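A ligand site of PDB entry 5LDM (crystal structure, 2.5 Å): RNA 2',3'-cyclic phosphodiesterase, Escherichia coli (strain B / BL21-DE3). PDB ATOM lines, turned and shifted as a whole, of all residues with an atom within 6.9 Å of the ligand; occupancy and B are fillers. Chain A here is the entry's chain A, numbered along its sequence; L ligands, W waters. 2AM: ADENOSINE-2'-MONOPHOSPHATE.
O1P of the ligand is in salt-bridge range of NH2 of Arg 131 (2.6 Å). A ring nitrogen (NE2) of His 126 lies within hydrogen-bond range of an oxygen (O2P) of the ligand (2.7 Å). A ring nitrogen (NE2) of His 44 lies within hydrogen-bond range of an oxygen (O3') of the ligand, 2.9 Å away. The side-chain hydroxyl of Thr 128 lies within hydrogen-bond range of an oxygen (O1P) of the ligand (2.9 Å). An oxygen (O3') of the ligand is in hydrogen-bond range of the side-chain hydroxyl of Thr 46 (2.9 Å).
OG1 of Thr 46 sits at hydrogen-bond distance from NE2 of His 44 (3.0 Å). O of Asn 42 lies within hydrogen-bond range of ND1 of His 44.
CE2 of Phe 9 touches C5' of the ligand, 3.8 Å away. Phe 49 touches the ligand. Tyr 167 touches the ligand. Hydrophobic or aromatic side chains that line the ligand: Phe 9, His 44, Phe 49, His 126 and Tyr 167. Eight residues have an atom within 4 Å of the ligand: Phe 9, His 44, Thr 46, Phe 49, His 126, Thr 128, Arg 131 and Tyr 167. The nearest printed residue that does not touch the ligand is Arg 7 (4.3 Å).
Water W1 lies within hydrogen-bond range of an oxygen (O1P) of the ligand (2.9 Å), the backbone NH of Thr 128 (3.1 Å) and the backbone carbonyl oxygen of His 44 (3.3 Å).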
ATOM      1  N   ARG A   7      15.793   2.432  18.635  1.00  0.00           N
ATOM      2  CA  ARG A   7      14.340   2.297  18.722  1.00  0.00           C
ATOM      3  C   ARG A   7      13.691   3.500  18.028  1.00  0.00           C
ATOM      4  O   ARG A   7      13.772   4.628  18.524  1.00  0.00           O
ATOM      5  CB  ARG A   7      13.899   2.229  20.186  1.00  0.00           C
ATOM      6  CG  ARG A   7      12.463   1.768  20.370  1.00  0.00           C
ATOM      7  CD  ARG A   7      12.103   1.635  21.853  1.00  0.00           C
ATOM      8  NE  ARG A   7      12.993   0.740  22.584  1.00  0.00           N
ATOM      9  CZ  ARG A   7      12.937  -0.595  22.532  1.00  0.00           C
ATOM     10  NH1 ARG A   7      13.814  -1.313  23.240  1.00  0.00           N
ATOM     11  NH2 ARG A   7      12.029  -1.214  21.786  1.00  0.00           N
ATOM     12  N   LEU A   8      13.080   3.259  16.869  1.00  0.00           N
ATOM     13  CA  LEU A   8      12.582   4.324  16.016  1.00  0.00           C
ATOM     14  C   LEU A   8      11.080   4.221  15.807  1.00  0.00           C
ATOM     15  O   LEU A   8      10.512   3.135  15.892  1.00  0.00           O
ATOM     16  CB  LEU A   8      13.274   4.290  14.657  1.00  0.00           C
ATOM     17  CG  LEU A   8      14.804   4.339  14.650  1.00  0.00           C
ATOM     18  CD1 LEU A   8      15.312   4.525  13.229  1.00  0.00           C
ATOM     19  CD2 LEU A   8      15.321   5.460  15.541  1.00  0.00           C
ATOM     20  N   PHE A   9      10.445   5.361  15.526  1.00  0.00           N
ATOM     21  CA  PHE A   9       9.021   5.409  15.229  1.00  0.00           C
ATOM     22  C   PHE A   9       8.662   6.698  14.466  1.00  0.00           C
ATOM     23  O   PHE A   9       9.231   7.755  14.723  1.00  0.00           O
ATOM     24  CB  PHE A   9       8.198   5.305  16.512  1.00  0.00           C
ATOM     25  CG  PHE A   9       8.339   6.504  17.418  1.00  0.00           C
ATOM     26  CD1 PHE A   9       7.469   7.582  17.314  1.00  0.00           C
ATOM     27  CD2 PHE A   9       9.318   6.543  18.387  1.00  0.00           C
ATOM     28  CE1 PHE A   9       7.595   8.676  18.158  1.00  0.00           C
ATOM     29  CE2 PHE A   9       9.456   7.639  19.225  1.00  0.00           C
ATOM     30  CZ  PHE A   9       8.599   8.703  19.109  1.00  0.00           C
ATOM     31  N   VAL A  38       2.644  11.896  30.944  1.00  0.00           N
ATOM     32  CA  VAL A  38       3.618  12.057  29.877  1.00  0.00           C
ATOM     33  C   VAL A  38       4.097  13.510  29.830  1.00  0.00           C
ATOM     34  O   VAL A  38       3.275  14.429  29.905  1.00  0.00           O
ATOM     35  CB  VAL A  38       3.016  11.654  28.504  1.00  0.00           C
ATOM     36  CG1 VAL A  38       4.002  11.909  27.372  1.00  0.00           C
ATOM     37  CG2 VAL A  38       2.594  10.205  28.522  1.00  0.00           C
ATOM     38  N   ASN A  42       6.807  15.280  25.071  1.00  0.00           N
ATOM     39  CA  ASN A  42       6.735  13.896  24.578  1.00  0.00           C
ATOM     40  C   ASN A  42       5.356  13.514  24.053  1.00  0.00           C
ATOM     41  O   ASN A  42       5.171  12.421  23.515  1.00  0.00           O
ATOM     42  CB  ASN A  42       7.171  12.905  25.653  1.00  0.00           C
ATOM     43  CG  ASN A  42       8.675  12.957  25.923  1.00  0.00           C
ATOM     44  OD1 ASN A  42       9.421  13.606  25.200  1.00  0.00           O
ATOM     45  ND2 ASN A  42       9.111  12.265  26.967  1.00  0.00           N
ATOM     46  N   HIS A  44       2.528  13.100  21.561  1.00  0.00           N
ATOM     47  CA  HIS A  44       2.579  12.893  20.114  1.00  0.00           C
ATOM     48  C   HIS A  44       1.596  11.806  19.737  1.00  0.00           C
ATOM     49  O   HIS A  44       1.039  11.120  20.609  1.00  0.00           O
ATOM     50  CB  HIS A  44       3.983  12.430  19.708  1.00  0.00           C
ATOM     51  CG  HIS A  44       4.299  11.047  20.187  1.00  0.00           C
ATOM     52  ND1 HIS A  44       4.952  10.808  21.376  1.00  0.00           N
ATOM     53  CD2 HIS A  44       3.998   9.836  19.665  1.00  0.00           C
ATOM     54  CE1 HIS A  44       5.057   9.501  21.562  1.00  0.00           C
ATOM     55  NE2 HIS A  44       4.489   8.892  20.533  1.00  0.00           N
ATOM     56  N   LEU A  45       1.412  11.623  18.436  1.00  0.00           N
ATOM     57  CA  LEU A  45       0.563  10.568  17.883  1.00  0.00           C
ATOM     58  C   LEU A  45       1.400   9.669  16.991  1.00  0.00           C
ATOM     59  O   LEU A  45       1.857  10.088  15.924  1.00  0.00           O
ATOM     60  CB  LEU A  45      -0.575  11.198  17.062  1.00  0.00           C
ATOM     61  CG  LEU A  45      -1.667  10.267  16.511  1.00  0.00           C
ATOM     62  CD1 LEU A  45      -2.934  11.051  16.303  1.00  0.00           C
ATOM     63  CD2 LEU A  45      -1.258   9.603  15.214  1.00  0.00           C
ATOM     64  N   THR A  46       1.614   8.439  17.428  1.00  0.00           N
ATOM     65  CA  THR A  46       2.463   7.522  16.684  1.00  0.00           C
ATOM     66  C   THR A  46       1.741   7.066  15.430  1.00  0.00           C
ATOM     67  O   THR A  46       0.543   6.762  15.461  1.00  0.00           O
ATOM     68  CB  THR A  46       2.854   6.308  17.516  1.00  0.00           C
ATOM     69  OG1 THR A  46       3.447   6.733  18.748  1.00  0.00           O
ATOM     70  CG2 THR A  46       3.848   5.440  16.753  1.00  0.00           C
ATOM     71  N   ALA A  48       3.576   4.805  13.308  1.00  0.00           N
ATOM     72  CA  ALA A  48       4.159   3.463  13.133  1.00  0.00           C
ATOM     73  C   ALA A  48       5.390   3.299  14.015  1.00  0.00           C
ATOM     74  O   ALA A  48       6.324   4.106  13.962  1.00  0.00           O
ATOM     75  CB  ALA A  48       4.526   3.235  11.671  1.00  0.00           C
ATOM     76  N   PHE A  49       5.380   2.245  14.830  1.00  0.00           N
ATOM     77  CA  PHE A  49       6.532   1.873  15.648  1.00  0.00           C
ATOM     78  C   PHE A  49       7.383   0.858  14.917  1.00  0.00           C
ATOM     79  O   PHE A  49       6.905  -0.203  14.498  1.00  0.00           O
ATOM     80  CB  PHE A  49       6.075   1.272  16.976  1.00  0.00           C
ATOM     81  CG  PHE A  49       7.214   0.911  17.891  1.00  0.00           C
ATOM     82  CD1 PHE A  49       7.902   1.901  18.575  1.00  0.00           C
ATOM     83  CD2 PHE A  49       7.602  -0.409  18.051  1.00  0.00           C
ATOM     84  CE1 PHE A  49       8.950   1.566  19.410  1.00  0.00           C
ATOM     85  CE2 PHE A  49       8.650  -0.744  18.886  1.00  0.00           C
ATOM     86  CZ  PHE A  49       9.326   0.247  19.563  1.00  0.00           C
ATOM     87  N   LEU A  50       8.663   1.170  14.772  1.00  0.00           N
ATOM     88  CA  LEU A  50       9.546   0.392  13.930  1.00  0.00           C
ATOM     89  C   LEU A  50      10.386  -0.573  14.767  1.00  0.00           C
ATOM     90  O   LEU A  50      10.847  -1.587  14.265  1.00  0.00           O
ATOM     91  CB  LEU A  50      10.441   1.324  13.129  1.00  0.00           C
ATOM     92  CG  LEU A  50       9.711   2.450  12.366  1.00  0.00           C
ATOM     93  CD1 LEU A  50      10.725   3.357  11.740  1.00  0.00           C
ATOM     94  CD2 LEU A  50       8.772   1.898  11.309  1.00  0.00           C
ATOM     95  N   GLY A  51      10.563  -0.241  16.046  1.00  0.00           N
ATOM     96  CA  GLY A  51      11.363  -1.072  16.931  1.00  0.00           C
ATOM     97  C   GLY A  51      12.835  -0.831  16.708  1.00  0.00           C
ATOM     98  O   GLY A  51      13.233   0.200  16.197  1.00  0.00           O
ATOM     99  N   TRP A  83      -7.473   2.646  27.967  1.00  0.00           N
ATOM    100  CA  TRP A  83      -7.274   1.214  27.737  1.00  0.00           C
ATOM    101  C   TRP A  83      -6.668   0.613  28.984  1.00  0.00           C
ATOM    102  O   TRP A  83      -5.531   0.893  29.333  1.00  0.00           O
ATOM    103  CB  TRP A  83      -6.349   0.998  26.543  1.00  0.00           C
ATOM    104  CG  TRP A  83      -6.924   1.473  25.236  1.00  0.00           C
ATOM    105  CD1 TRP A  83      -8.245   1.527  24.888  1.00  0.00           C
ATOM    106  CD2 TRP A  83      -6.198   1.997  24.113  1.00  0.00           C
ATOM    107  NE1 TRP A  83      -8.384   2.027  23.621  1.00  0.00           N
ATOM    108  CE2 TRP A  83      -7.142   2.327  23.123  1.00  0.00           C
ATOM    109  CE3 TRP A  83      -4.842   2.212  23.848  1.00  0.00           C
ATOM    110  CZ2 TRP A  83      -6.776   2.854  21.887  1.00  0.00           C
ATOM    111  CZ3 TRP A  83      -4.484   2.743  22.613  1.00  0.00           C
ATOM    112  CH2 TRP A  83      -5.448   3.053  21.655  1.00  0.00           C
ATOM    113  N   SER A  86      -3.498  -1.915  28.510  1.00  0.00           N
ATOM    114  CA  SER A  86      -2.265  -1.167  28.252  1.00  0.00           C
ATOM    115  C   SER A  86      -1.969  -0.223  29.408  1.00  0.00           C
ATOM    116  O   SER A  86      -0.857   0.310  29.520  1.00  0.00           O
ATOM    117  CB  SER A  86      -2.395  -0.360  26.970  1.00  0.00           C
ATOM    118  OG  SER A  86      -3.042  -1.099  25.946  1.00  0.00           O
ATOM    119  N   VAL A  88      -3.203   2.876  29.967  1.00  0.00           N
ATOM    120  CA  VAL A  88      -3.004   4.260  29.528  1.00  0.00           C
ATOM    121  C   VAL A  88      -4.311   5.027  29.432  1.00  0.00           C
ATOM    122  O   VAL A  88      -5.380   4.448  29.250  1.00  0.00           O
ATOM    123  CB  VAL A  88      -2.319   4.337  28.152  1.00  0.00           C
ATOM    124  CG1 VAL A  88      -0.890   3.831  28.230  1.00  0.00           C
ATOM    125  CG2 VAL A  88      -3.110   3.556  27.119  1.00  0.00           C
ATOM    126  N   SER A 119       2.374  -4.256  14.307  1.00  0.00           N
ATOM    127  CA  SER A 119       1.524  -4.047  15.469  1.00  0.00           C
ATOM    128  C   SER A 119       0.795  -5.308  15.899  1.00  0.00           C
ATOM    129  O   SER A 119       0.593  -5.535  17.090  1.00  0.00           O
ATOM    130  CB  SER A 119       0.495  -2.962  15.157  1.00  0.00           C
ATOM    131  OG  SER A 119       0.896  -1.709  15.695  1.00  0.00           O
ATOM    132  N   HIS A 126      -3.980   7.745  18.482  1.00  0.00           N
ATOM    133  CA  HIS A 126      -4.189   8.241  19.833  1.00  0.00           C
ATOM    134  C   HIS A 126      -2.942   8.974  20.327  1.00  0.00           C
ATOM    135  O   HIS A 126      -1.846   8.775  19.797  1.00  0.00           O
ATOM    136  CB  HIS A 126      -4.479   7.066  20.767  1.00  0.00           C
ATOM    137  CG  HIS A 126      -3.300   6.173  20.986  1.00  0.00           C
ATOM    138  ND1 HIS A 126      -2.922   5.206  20.074  1.00  0.00           N
ATOM    139  CD2 HIS A 126      -2.383   6.126  21.979  1.00  0.00           C
ATOM    140  CE1 HIS A 126      -1.836   4.588  20.513  1.00  0.00           C
ATOM    141  NE2 HIS A 126      -1.491   5.131  21.667  1.00  0.00           N
ATOM    142  N   ILE A 127      -3.132   9.845  21.309  1.00  0.00           N
ATOM    143  CA  ILE A 127      -2.034  10.497  22.010  1.00  0.00           C
ATOM    144  C   ILE A 127      -2.114  10.094  23.463  1.00  0.00           C
ATOM    145  O   ILE A 127      -3.131  10.333  24.118  1.00  0.00           O
ATOM    146  CB  ILE A 127      -2.102  12.034  21.908  1.00  0.00           C
ATOM    147  CG1 ILE A 127      -1.920  12.504  20.470  1.00  0.00           C
ATOM    148  CG2 ILE A 127      -1.037  12.680  22.797  1.00  0.00           C
ATOM    149  CD1 ILE A 127      -3.200  12.594  19.709  1.00  0.00           C
ATOM    150  N   THR A 128      -1.039   9.515  23.984  1.00  0.00           N
ATOM    151  CA  THR A 128      -1.044   9.025  25.350  1.00  0.00           C
ATOM    152  C   THR A 128      -0.735  10.127  26.348  1.00  0.00           C
ATOM    153  O   THR A 128       0.297  10.796  26.246  1.00  0.00           O
ATOM    154  CB  THR A 128      -0.039   7.864  25.506  1.00  0.00           C
ATOM    155  OG1 THR A 128      -0.444   6.778  24.666  1.00  0.00           O
ATOM    156  CG2 THR A 128       0.025   7.371  26.951  1.00  0.00           C
ATOM    157  N   ARG A 131       0.451   7.131  31.712  1.00  0.00           N
ATOM    158  CA  ARG A 131       0.961   5.769  31.606  1.00  0.00           C
ATOM    159  C   ARG A 131       0.869   5.079  32.968  1.00  0.00           C
ATOM    160  O   ARG A 131       0.828   5.755  34.003  1.00  0.00           O
ATOM    161  CB  ARG A 131       2.403   5.765  31.084  1.00  0.00           C
ATOM    162  CG  ARG A 131       2.536   6.323  29.661  1.00  0.00           C
ATOM    163  CD  ARG A 131       3.872   5.945  29.014  1.00  0.00           C
ATOM    164  NE  ARG A 131       3.988   6.497  27.662  1.00  0.00           N
ATOM    165  CZ  ARG A 131       3.548   5.882  26.565  1.00  0.00           C
ATOM    166  NH1 ARG A 131       2.973   4.693  26.632  1.00  0.00           N
ATOM    167  NH2 ARG A 131       3.686   6.466  25.381  1.00  0.00           N
ATOM    168  N   SER A 158      13.719   6.878  20.056  1.00  0.00           N
ATOM    169  CA  SER A 158      13.349   6.786  21.462  1.00  0.00           C
ATOM    170  C   SER A 158      14.598   6.439  22.271  1.00  0.00           C
ATOM    171  O   SER A 158      15.362   5.559  21.900  1.00  0.00           O
ATOM    172  CB  SER A 158      12.273   5.712  21.655  1.00  0.00           C
ATOM    173  OG  SER A 158      11.904   5.594  23.026  1.00  0.00           O
ATOM    174  N   THR A 165      12.388   9.593  29.659  1.00  0.00           N
ATOM    175  CA  THR A 165      12.271   9.133  28.283  1.00  0.00           C
ATOM    176  C   THR A 165      12.425  10.336  27.350  1.00  0.00           C
ATOM    177  O   THR A 165      11.789  11.369  27.560  1.00  0.00           O
ATOM    178  CB  THR A 165      10.924   8.436  28.060  1.00  0.00           C
ATOM    179  OG1 THR A 165      10.850   7.275  28.887  1.00  0.00           O
ATOM    180  CG2 THR A 165      10.765   8.022  26.609  1.00  0.00           C
ATOM    181  N   TYR A 167      12.711  11.817  23.195  1.00  0.00           N
ATOM    182  CA  TYR A 167      12.430  11.601  21.785  1.00  0.00           C
ATOM    183  C   TYR A 167      13.263  12.558  20.939  1.00  0.00           C
ATOM    184  O   TYR A 167      13.032  13.762  20.948  1.00  0.00           O
ATOM    185  CB  TYR A 167      10.945  11.821  21.478  1.00  0.00           C
ATOM    186  CG  TYR A 167      10.016  10.845  22.160  1.00  0.00           C
ATOM    187  CD1 TYR A 167      10.402   9.539  22.410  1.00  0.00           C
ATOM    188  CD2 TYR A 167       8.746  11.238  22.562  1.00  0.00           C
ATOM    189  CE1 TYR A 167       9.556   8.636  23.028  1.00  0.00           C
ATOM    190  CE2 TYR A 167       7.886  10.350  23.192  1.00  0.00           C
ATOM    191  CZ  TYR A 167       8.294   9.044  23.420  1.00  0.00           C
ATOM    192  OH  TYR A 167       7.450   8.162  24.050  1.00  0.00           O
HETATM  193  P   2AM L   1       1.946   4.331  23.193  1.00  0.00           P
HETATM  194  O1P 2AM L   1       2.042   5.800  23.509  1.00  0.00           O
HETATM  195  O2P 2AM L   1       0.504   3.945  22.966  1.00  0.00           O
HETATM  196  O3P 2AM L   1       2.518   3.526  24.340  1.00  0.00           O
HETATM  197  C5' 2AM L   1       7.271   5.676  21.570  1.00  0.00           C
HETATM  198  O5' 2AM L   1       7.736   4.612  22.364  1.00  0.00           O
HETATM  199  C4' 2AM L   1       5.940   5.307  20.931  1.00  0.00           C
HETATM  200  O4' 2AM L   1       5.995   4.011  20.371  1.00  0.00           O
HETATM  201  C3' 2AM L   1       4.820   5.300  21.964  1.00  0.00           C
HETATM  202  O3' 2AM L   1       3.893   6.306  21.631  1.00  0.00           O
HETATM  203  C2' 2AM L   1       4.207   3.910  21.895  1.00  0.00           C
HETATM  204  O2' 2AM L   1       2.808   3.988  21.874  1.00  0.00           O
HETATM  205  C1' 2AM L   1       4.784   3.322  20.615  1.00  0.00           C
HETATM  206  N9  2AM L   1       5.016   1.853  20.667  1.00  0.00           N
HETATM  207  C8  2AM L   1       4.236   0.906  20.052  1.00  0.00           C
HETATM  208  N7  2AM L   1       4.769  -0.314  20.300  1.00  0.00           N
HETATM  209  C5  2AM L   1       5.878  -0.163  21.055  1.00  0.00           C
HETATM  210  C6  2AM L   1       6.794  -1.077  21.576  1.00  0.00           C
HETATM  211  N6  2AM L   1       6.648  -2.383  21.358  1.00  0.00           N
HETATM  212  N1  2AM L   1       7.849  -0.607  22.329  1.00  0.00           N
HETATM  213  C2  2AM L   1       8.001   0.747  22.544  1.00  0.00           C
HETATM  214  N3  2AM L   1       7.094   1.640  22.017  1.00  0.00           N
HETATM  215  C4  2AM L   1       6.050   1.202  21.280  1.00  0.00           C
HETATM  216  O   HOH W   1       1.326   8.387  22.414  1.00  0.00           O
